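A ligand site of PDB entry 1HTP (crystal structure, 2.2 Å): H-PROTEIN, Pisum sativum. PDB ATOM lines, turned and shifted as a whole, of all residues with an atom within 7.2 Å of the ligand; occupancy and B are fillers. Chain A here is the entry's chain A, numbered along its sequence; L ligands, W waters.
Water W1 lies within hydrogen-bond range of S3 of the ligand and OE1 of Glu 127.
The side-chain carboxylate of Glu 14 lies within hydrogen-bond range of the side-chain hydroxyl of Ser 12 (2.7 Å). The backbone NH (N) of Asn 69 sits at hydrogen-bond distance from the side-chain carboxylate (OE2) of Glu 14. NE2 of His 13 sits at hydrogen-bond distance from OE1 of Glu 127, at 2.9 Å. The backbone carbonyl oxygen of Pro 11 sits at hydrogen-bond distance from a ring nitrogen (NE2) of His 13, at 3.4 Å. The backbone carbonyl oxygen (O) of His 13 lies within hydrogen-bond range of the backbone NH (N) of Thr 28. OG1 of Thr 28 sits at hydrogen-bond distance from N of Ala 31 (3.4 Å). O of Leu 35 lies within hydrogen-bond range of OG of Ser 61, 2.8 Å away. The backbone NH (N) of Ala 64 lies within hydrogen-bond range of the side-chain hydroxyl (OG) of Ser 61 (2.7 Å).
Residues that only touch the ligand: His 34 (3.0 Å), Ala 31 (3.5 Å), Ser 66 (3.5 Å), Leu 35 (3.6 Å), Ala 64 (3.6 Å), Ile 27 (3.8 Å) and Val 59 (3.9 Å). Hydrophobic or aromatic side chains that line the ligand: His 13, Ile 27, Ala 31, His 34, Leu 35, Val 59 and Ala 64. Within 4 Å of the ligand: Ser 12, His 13, Glu 14, Ile 27, Ala 31, His 34, Leu 35, Val 59, Lys 63, Ala 64, Ser 66, Asp 67 and Glu 127. The nearest printed residue that does not touch the ligand is Val 68 (4.1 Å).
NZ of Lys 63 is covalently linked to C1 of the ligand (1.3 Å). A nitrogen (N1) of the ligand is in salt-bridge range of the side-chain carboxylate of Glu 14, at 2.8 Å. A ring nitrogen (NE2) of His 13 lies within hydrogen-bond range of an oxygen (O2) of the ligand (2.9 Å). The backbone carbonyl oxygen (O) of Ser 12 is in hydrogen-bond range of a nitrogen (N1) of the ligand (2.9 Å). A nitrogen (N1) of the ligand is in hydrogen-bond range of the backbone carbonyl oxygen of Asp 67, 2.9 Å away. OE2 of Glu 127 sits at hydrogen-bond distance from O2 of the ligand (3.1 Å).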
ATOM      1  N   PRO A  11     -19.568   9.372   1.700  1.00  0.00           N
ATOM      2  CA  PRO A  11     -18.684   8.478   0.969  1.00  0.00           C
ATOM      3  C   PRO A  11     -18.912   7.008   1.286  1.00  0.00           C
ATOM      4  O   PRO A  11     -18.730   6.127   0.446  1.00  0.00           O
ATOM      5  CB  PRO A  11     -17.296   8.916   1.331  1.00  0.00           C
ATOM      6  CG  PRO A  11     -17.461  10.382   1.414  1.00  0.00           C
ATOM      7  CD  PRO A  11     -18.776  10.475   2.195  1.00  0.00           C
ATOM      8  N   SER A  12     -19.354   6.699   2.497  1.00  0.00           N
ATOM      9  CA  SER A  12     -19.514   5.318   2.888  1.00  0.00           C
ATOM     10  C   SER A  12     -20.833   4.745   2.413  1.00  0.00           C
ATOM     11  O   SER A  12     -21.180   3.654   2.798  1.00  0.00           O
ATOM     12  CB  SER A  12     -19.347   5.248   4.389  1.00  0.00           C
ATOM     13  OG  SER A  12     -19.918   6.403   5.066  1.00  0.00           O
ATOM     14  N   HIS A  13     -21.584   5.437   1.539  1.00  0.00           N
ATOM     15  CA  HIS A  13     -22.795   4.949   0.863  1.00  0.00           C
ATOM     16  C   HIS A  13     -24.079   4.886   1.645  1.00  0.00           C
ATOM     17  O   HIS A  13     -24.920   4.011   1.495  1.00  0.00           O
ATOM     18  CB  HIS A  13     -22.471   3.584   0.201  1.00  0.00           C
ATOM     19  CG  HIS A  13     -21.353   3.759  -0.835  1.00  0.00           C
ATOM     20  ND1 HIS A  13     -21.346   4.553  -1.915  1.00  0.00           N
ATOM     21  CD2 HIS A  13     -20.118   3.188  -0.772  1.00  0.00           C
ATOM     22  CE1 HIS A  13     -20.165   4.467  -2.464  1.00  0.00           C
ATOM     23  NE2 HIS A  13     -19.428   3.651  -1.788  1.00  0.00           N
ATOM     24  N   GLU A  14     -24.303   5.956   2.401  1.00  0.00           N
ATOM     25  CA  GLU A  14     -25.535   6.181   3.161  1.00  0.00           C
ATOM     26  C   GLU A  14     -26.091   7.491   2.701  1.00  0.00           C
ATOM     27  O   GLU A  14     -25.280   8.386   2.424  1.00  0.00           O
ATOM     28  CB  GLU A  14     -25.321   6.326   4.646  1.00  0.00           C
ATOM     29  CG  GLU A  14     -24.777   5.072   5.243  1.00  0.00           C
ATOM     30  CD  GLU A  14     -23.295   5.105   5.443  1.00  0.00           C
ATOM     31  OE1 GLU A  14     -22.621   6.098   5.167  1.00  0.00           O
ATOM     32  OE2 GLU A  14     -22.802   4.106   5.935  1.00  0.00           O
ATOM     33  N   GLY A  26     -30.720   5.790   5.183  1.00  0.00           N
ATOM     34  CA  GLY A  26     -30.647   4.443   4.617  1.00  0.00           C
ATOM     35  C   GLY A  26     -29.326   4.329   3.833  1.00  0.00           C
ATOM     36  O   GLY A  26     -28.526   5.268   3.845  1.00  0.00           O
ATOM     37  N   ILE A  27     -29.013   3.181   3.218  1.00  0.00           N
ATOM     38  CA  ILE A  27     -27.833   3.018   2.350  1.00  0.00           C
ATOM     39  C   ILE A  27     -28.262   3.098   0.863  1.00  0.00           C
ATOM     40  O   ILE A  27     -29.407   2.815   0.477  1.00  0.00           O
ATOM     41  CB  ILE A  27     -27.154   1.675   2.569  1.00  0.00           C
ATOM     42  CG1 ILE A  27     -28.079   0.530   2.161  1.00  0.00           C
ATOM     43  CG2 ILE A  27     -26.732   1.608   4.004  1.00  0.00           C
ATOM     44  CD1 ILE A  27     -27.358  -0.803   2.146  1.00  0.00           C
ATOM     45  N   THR A  28     -27.387   3.456  -0.040  1.00  0.00           N
ATOM     46  CA  THR A  28     -27.809   3.698  -1.399  1.00  0.00           C
ATOM     47  C   THR A  28     -27.980   2.440  -2.260  1.00  0.00           C
ATOM     48  O   THR A  28     -27.632   1.319  -1.880  1.00  0.00           O
ATOM     49  CB  THR A  28     -26.785   4.670  -1.974  1.00  0.00           C
ATOM     50  OG1 THR A  28     -25.555   3.968  -1.978  1.00  0.00           O
ATOM     51  CG2 THR A  28     -26.615   5.972  -1.172  1.00  0.00           C
ATOM     52  N   HIS A  30     -26.235   1.710  -4.765  1.00  0.00           N
ATOM     53  CA  HIS A  30     -24.867   1.294  -4.989  1.00  0.00           C
ATOM     54  C   HIS A  30     -24.467   0.352  -3.888  1.00  0.00           C
ATOM     55  O   HIS A  30     -24.011  -0.752  -4.154  1.00  0.00           O
ATOM     56  CB  HIS A  30     -23.906   2.516  -4.995  1.00  0.00           C
ATOM     57  CG  HIS A  30     -22.425   2.194  -5.206  1.00  0.00           C
ATOM     58  ND1 HIS A  30     -21.465   2.123  -4.284  1.00  0.00           N
ATOM     59  CD2 HIS A  30     -21.894   1.895  -6.422  1.00  0.00           C
ATOM     60  CE1 HIS A  30     -20.380   1.781  -4.920  1.00  0.00           C
ATOM     61  NE2 HIS A  30     -20.634   1.642  -6.186  1.00  0.00           N
ATOM     62  N   ALA A  31     -24.692   0.772  -2.634  1.00  0.00           N
ATOM     63  CA  ALA A  31     -24.320   0.008  -1.469  1.00  0.00           C
ATOM     64  C   ALA A  31     -25.021  -1.333  -1.483  1.00  0.00           C
ATOM     65  O   ALA A  31     -24.314  -2.329  -1.382  1.00  0.00           O
ATOM     66  CB  ALA A  31     -24.706   0.778  -0.216  1.00  0.00           C
ATOM     67  N   GLN A  32     -26.333  -1.443  -1.698  1.00  0.00           N
ATOM     68  CA  GLN A  32     -27.029  -2.738  -1.642  1.00  0.00           C
ATOM     69  C   GLN A  32     -26.538  -3.680  -2.755  1.00  0.00           C
ATOM     70  O   GLN A  32     -26.183  -4.837  -2.543  1.00  0.00           O
ATOM     71  CB  GLN A  32     -28.551  -2.510  -1.718  1.00  0.00           C
ATOM     72  CG  GLN A  32     -29.266  -1.986  -2.972  1.00  0.00           C
ATOM     73  CD  GLN A  32     -29.497  -2.979  -4.126  1.00  0.00           C
ATOM     74  OE1 GLN A  32     -29.454  -4.186  -3.929  1.00  0.00           O
ATOM     75  NE2 GLN A  32     -29.670  -2.614  -5.384  1.00  0.00           N
ATOM     76  N   ASP A  33     -26.339  -3.137  -3.960  1.00  0.00           N
ATOM     77  CA  ASP A  33     -25.784  -3.867  -5.102  1.00  0.00           C
ATOM     78  C   ASP A  33     -24.469  -4.562  -4.843  1.00  0.00           C
ATOM     79  O   ASP A  33     -24.252  -5.702  -5.209  1.00  0.00           O
ATOM     80  CB  ASP A  33     -25.603  -2.891  -6.221  1.00  0.00           C
ATOM     81  CG  ASP A  33     -26.093  -3.408  -7.525  1.00  0.00           C
ATOM     82  OD1 ASP A  33     -26.956  -4.279  -7.595  1.00  0.00           O
ATOM     83  OD2 ASP A  33     -25.596  -2.879  -8.488  1.00  0.00           O
ATOM     84  N   HIS A  34     -23.564  -3.822  -4.240  1.00  0.00           N
ATOM     85  CA  HIS A  34     -22.273  -4.360  -3.854  1.00  0.00           C
ATOM     86  C   HIS A  34     -22.340  -5.260  -2.625  1.00  0.00           C
ATOM     87  O   HIS A  34     -21.396  -6.001  -2.374  1.00  0.00           O
ATOM     88  CB  HIS A  34     -21.308  -3.231  -3.571  1.00  0.00           C
ATOM     89  CG  HIS A  34     -20.821  -2.612  -4.859  1.00  0.00           C
ATOM     90  ND1 HIS A  34     -21.493  -1.903  -5.748  1.00  0.00           N
ATOM     91  CD2 HIS A  34     -19.521  -2.643  -5.268  1.00  0.00           C
ATOM     92  CE1 HIS A  34     -20.642  -1.496  -6.653  1.00  0.00           C
ATOM     93  NE2 HIS A  34     -19.453  -1.932  -6.364  1.00  0.00           N
ATOM     94  N   LEU A  35     -23.434  -5.261  -1.865  1.00  0.00           N
ATOM     95  CA  LEU A  35     -23.571  -6.081  -0.656  1.00  0.00           C
ATOM     96  C   LEU A  35     -24.129  -7.424  -1.045  1.00  0.00           C
ATOM     97  O   LEU A  35     -23.763  -8.427  -0.418  1.00  0.00           O
ATOM     98  CB  LEU A  35     -24.533  -5.420   0.332  1.00  0.00           C
ATOM     99  CG  LEU A  35     -24.007  -4.499   1.369  1.00  0.00           C
ATOM    100  CD1 LEU A  35     -25.175  -3.774   2.007  1.00  0.00           C
ATOM    101  CD2 LEU A  35     -23.243  -5.298   2.426  1.00  0.00           C
ATOM    102  N   GLY A  36     -25.026  -7.462  -1.998  1.00  0.00           N
ATOM    103  CA  GLY A  36     -25.613  -8.702  -2.385  1.00  0.00           C
ATOM    104  C   GLY A  36     -26.887  -8.804  -1.599  1.00  0.00           C
ATOM    105  O   GLY A  36     -27.409  -7.788  -1.156  1.00  0.00           O
ATOM    106  N   VAL A  59     -25.266  -3.946   8.508  1.00  0.00           N
ATOM    107  CA  VAL A  59     -26.122  -4.636   7.563  1.00  0.00           C
ATOM    108  C   VAL A  59     -25.308  -5.879   7.180  1.00  0.00           C
ATOM    109  O   VAL A  59     -24.082  -5.823   6.963  1.00  0.00           O
ATOM    110  CB  VAL A  59     -26.457  -3.584   6.414  1.00  0.00           C
ATOM    111  CG1 VAL A  59     -25.249  -3.009   5.727  1.00  0.00           C
ATOM    112  CG2 VAL A  59     -27.317  -4.288   5.403  1.00  0.00           C
ATOM    113  N   SER A  61     -25.021  -9.130   4.737  1.00  0.00           N
ATOM    114  CA  SER A  61     -25.454  -9.744   3.498  1.00  0.00           C
ATOM    115  C   SER A  61     -24.973 -11.189   3.439  1.00  0.00           C
ATOM    116  O   SER A  61     -24.262 -11.629   4.351  1.00  0.00           O
ATOM    117  CB  SER A  61     -24.888  -8.994   2.311  1.00  0.00           C
ATOM    118  OG  SER A  61     -23.467  -9.018   2.307  1.00  0.00           O
ATOM    119  N   LYS A  63     -22.632 -12.121   1.716  1.00  0.00           N
ATOM    120  CA  LYS A  63     -21.205 -12.055   1.632  1.00  0.00           C
ATOM    121  C   LYS A  63     -20.491 -11.095   2.551  1.00  0.00           C
ATOM    122  O   LYS A  63     -19.258 -11.227   2.684  1.00  0.00           O
ATOM    123  CB  LYS A  63     -20.827 -11.693   0.230  1.00  0.00           C
ATOM    124  CG  LYS A  63     -21.245 -10.288  -0.227  1.00  0.00           C
ATOM    125  CD  LYS A  63     -20.788 -10.086  -1.662  1.00  0.00           C
ATOM    126  CE  LYS A  63     -19.386  -9.560  -1.545  1.00  0.00           C
ATOM    127  NZ  LYS A  63     -19.574  -8.165  -1.350  1.00  0.00           N
ATOM    128  N   ALA A  64     -21.116 -10.116   3.207  1.00  0.00           N
ATOM    129  CA  ALA A  64     -20.347  -9.164   4.017  1.00  0.00           C
ATOM    130  C   ALA A  64     -21.156  -8.741   5.208  1.00  0.00           C
ATOM    131  O   ALA A  64     -22.338  -9.068   5.272  1.00  0.00           O
ATOM    132  CB  ALA A  64     -20.019  -7.893   3.234  1.00  0.00           C
ATOM    133  N   THR A  65     -20.543  -8.088   6.178  1.00  0.00           N
ATOM    134  CA  THR A  65     -21.269  -7.447   7.256  1.00  0.00           C
ATOM    135  C   THR A  65     -20.669  -6.057   7.267  1.00  0.00           C
ATOM    136  O   THR A  65     -19.464  -5.971   7.519  1.00  0.00           O
ATOM    137  CB  THR A  65     -21.012  -8.155   8.568  1.00  0.00           C
ATOM    138  OG1 THR A  65     -21.476  -9.471   8.406  1.00  0.00           O
ATOM    139  CG2 THR A  65     -21.753  -7.524   9.721  1.00  0.00           C
ATOM    140  N   SER A  66     -21.366  -4.970   6.930  1.00  0.00           N
ATOM    141  CA  SER A  66     -20.750  -3.659   7.015  1.00  0.00           C
ATOM    142  C   SER A  66     -21.491  -2.780   8.019  1.00  0.00           C
ATOM    143  O   SER A  66     -22.681  -2.954   8.343  1.00  0.00           O
ATOM    144  CB  SER A  66     -20.740  -2.905   5.664  1.00  0.00           C
ATOM    145  OG  SER A  66     -21.105  -3.762   4.592  1.00  0.00           O
ATOM    146  N   ASP A  67     -20.726  -1.827   8.521  1.00  0.00           N
ATOM    147  CA  ASP A  67     -21.223  -0.802   9.415  1.00  0.00           C
ATOM    148  C   ASP A  67     -22.008   0.174   8.605  1.00  0.00           C
ATOM    149  O   ASP A  67     -21.610   0.418   7.471  1.00  0.00           O
ATOM    150  CB  ASP A  67     -20.076  -0.001  10.065  1.00  0.00           C
ATOM    151  CG  ASP A  67     -19.253  -0.718  11.116  1.00  0.00           C
ATOM    152  OD1 ASP A  67     -19.772  -1.641  11.749  1.00  0.00           O
ATOM    153  OD2 ASP A  67     -18.103  -0.334  11.328  1.00  0.00           O
ATOM    154  N   VAL A  68     -23.065   0.737   9.157  1.00  0.00           N
ATOM    155  CA  VAL A  68     -23.749   1.788   8.462  1.00  0.00           C
ATOM    156  C   VAL A  68     -23.488   2.935   9.395  1.00  0.00           C
ATOM    157  O   VAL A  68     -23.854   2.848  10.567  1.00  0.00           O
ATOM    158  CB  VAL A  68     -25.215   1.540   8.374  1.00  0.00           C
ATOM    159  CG1 VAL A  68     -25.787   2.582   7.449  1.00  0.00           C
ATOM    160  CG2 VAL A  68     -25.508   0.169   7.886  1.00  0.00           C
ATOM    161  N   ASN A  69     -22.843   3.993   8.917  1.00  0.00           N
ATOM    162  CA  ASN A  69     -22.588   5.180   9.723  1.00  0.00           C
ATOM    163  C   ASN A  69     -23.609   6.257   9.490  1.00  0.00           C
ATOM    164  O   ASN A  69     -24.284   6.337   8.447  1.00  0.00           O
ATOM    165  CB  ASN A  69     -21.239   5.756   9.417  1.00  0.00           C
ATOM    166  CG  ASN A  69     -20.187   4.685   9.593  1.00  0.00           C
ATOM    167  OD1 ASN A  69     -20.292   3.734  10.377  1.00  0.00           O
ATOM    168  ND2 ASN A  69     -19.151   4.775   8.804  1.00  0.00           N
ATOM    169  N   MET A 100     -33.619   3.068   7.150  1.00  0.00           N
ATOM    170  CA  MET A 100     -33.222   2.430   8.392  1.00  0.00           C
ATOM    171  C   MET A 100     -33.638   3.135   9.684  1.00  0.00           C
ATOM    172  O   MET A 100     -34.241   2.490  10.542  1.00  0.00           O
ATOM    173  CB  MET A 100     -31.707   2.227   8.356  1.00  0.00           C
ATOM    174  CG  MET A 100     -31.397   1.286   7.195  1.00  0.00           C
ATOM    175  SD  MET A 100     -29.619   1.225   7.001  1.00  0.00           S
ATOM    176  CE  MET A 100     -29.427  -0.500   6.742  1.00  0.00           C
ATOM    177  N   PHE A 123     -18.341  10.022  -7.671  1.00  0.00           N
ATOM    178  CA  PHE A 123     -17.467   9.257  -6.810  1.00  0.00           C
ATOM    179  C   PHE A 123     -17.730   7.793  -6.987  1.00  0.00           C
ATOM    180  O   PHE A 123     -16.827   6.989  -6.873  1.00  0.00           O
ATOM    181  CB  PHE A 123     -17.716   9.706  -5.428  1.00  0.00           C
ATOM    182  CG  PHE A 123     -17.164   8.760  -4.403  1.00  0.00           C
ATOM    183  CD1 PHE A 123     -15.781   8.646  -4.184  1.00  0.00           C
ATOM    184  CD2 PHE A 123     -18.101   8.032  -3.652  1.00  0.00           C
ATOM    185  CE1 PHE A 123     -15.331   7.767  -3.201  1.00  0.00           C
ATOM    186  CE2 PHE A 123     -17.626   7.171  -2.686  1.00  0.00           C
ATOM    187  CZ  PHE A 123     -16.251   7.037  -2.464  1.00  0.00           C
ATOM    188  N   GLU A 127     -15.121   4.935  -8.154  1.00  0.00           N
ATOM    189  CA  GLU A 127     -14.942   3.673  -7.461  1.00  0.00           C
ATOM    190  C   GLU A 127     -15.106   2.462  -8.343  1.00  0.00           C
ATOM    191  O   GLU A 127     -14.342   1.512  -8.194  1.00  0.00           O
ATOM    192  CB  GLU A 127     -15.912   3.491  -6.287  1.00  0.00           C
ATOM    193  CG  GLU A 127     -15.398   4.230  -5.058  1.00  0.00           C
ATOM    194  CD  GLU A 127     -16.094   3.825  -3.777  1.00  0.00           C
ATOM    195  OE1 GLU A 127     -17.322   3.673  -3.806  1.00  0.00           O
ATOM    196  OE2 GLU A 127     -15.399   3.648  -2.776  1.00  0.00           O
HETATM  197  C1  LIG L   1     -18.682  -7.434  -0.706  1.00  0.00           C
HETATM  198  O1  LIG L   1     -17.637  -7.931  -0.285  1.00  0.00           O
HETATM  199  C2  LIG L   1     -19.048  -5.956  -0.537  1.00  0.00           C
HETATM  200  C3  LIG L   1     -18.938  -5.353   0.864  1.00  0.00           C
HETATM  201  C4  LIG L   1     -20.061  -4.344   1.036  1.00  0.00           C
HETATM  202  C5  LIG L   1     -19.657  -2.984   0.512  1.00  0.00           C
HETATM  203  C6  LIG L   1     -20.771  -1.942   0.463  1.00  0.00           C
HETATM  204  C7  LIG L   1     -21.260  -1.607   1.858  1.00  0.00           C
HETATM  205  C8  LIG L   1     -22.372  -0.553   2.000  1.00  0.00           C
HETATM  206  S1  LIG L   1     -23.160  -0.407   3.652  1.00  0.00           S
HETATM  207  C9  LIG L   1     -22.952   1.361   3.933  1.00  0.00           C
HETATM  208  N1  LIG L   1     -21.860   1.678   4.841  1.00  0.00           N
HETATM  209  S2  LIG L   1     -20.167  -0.422  -0.298  1.00  0.00           S
HETATM  210  S3  LIG L   1     -18.899  -0.646  -1.880  1.00  0.00           S
HETATM  211  C10 LIG L   1     -17.235  -0.572  -1.200  1.00  0.00           C
HETATM  212  C11 LIG L   1     -17.014   0.644  -0.327  1.00  0.00           C
HETATM  213  O2  LIG L   1     -17.282   1.879  -0.998  1.00  0.00           O
HETATM  214  O   HOH W   1     -17.825   0.447  -4.360  1.00  0.00           O
HETATM  215  O   HOH W   2     -15.578  -3.365  -1.039  1.00  0.00           O
HETATM  216  O   HOH W   3     -18.886   0.581   4.709  1.00  0.00           O
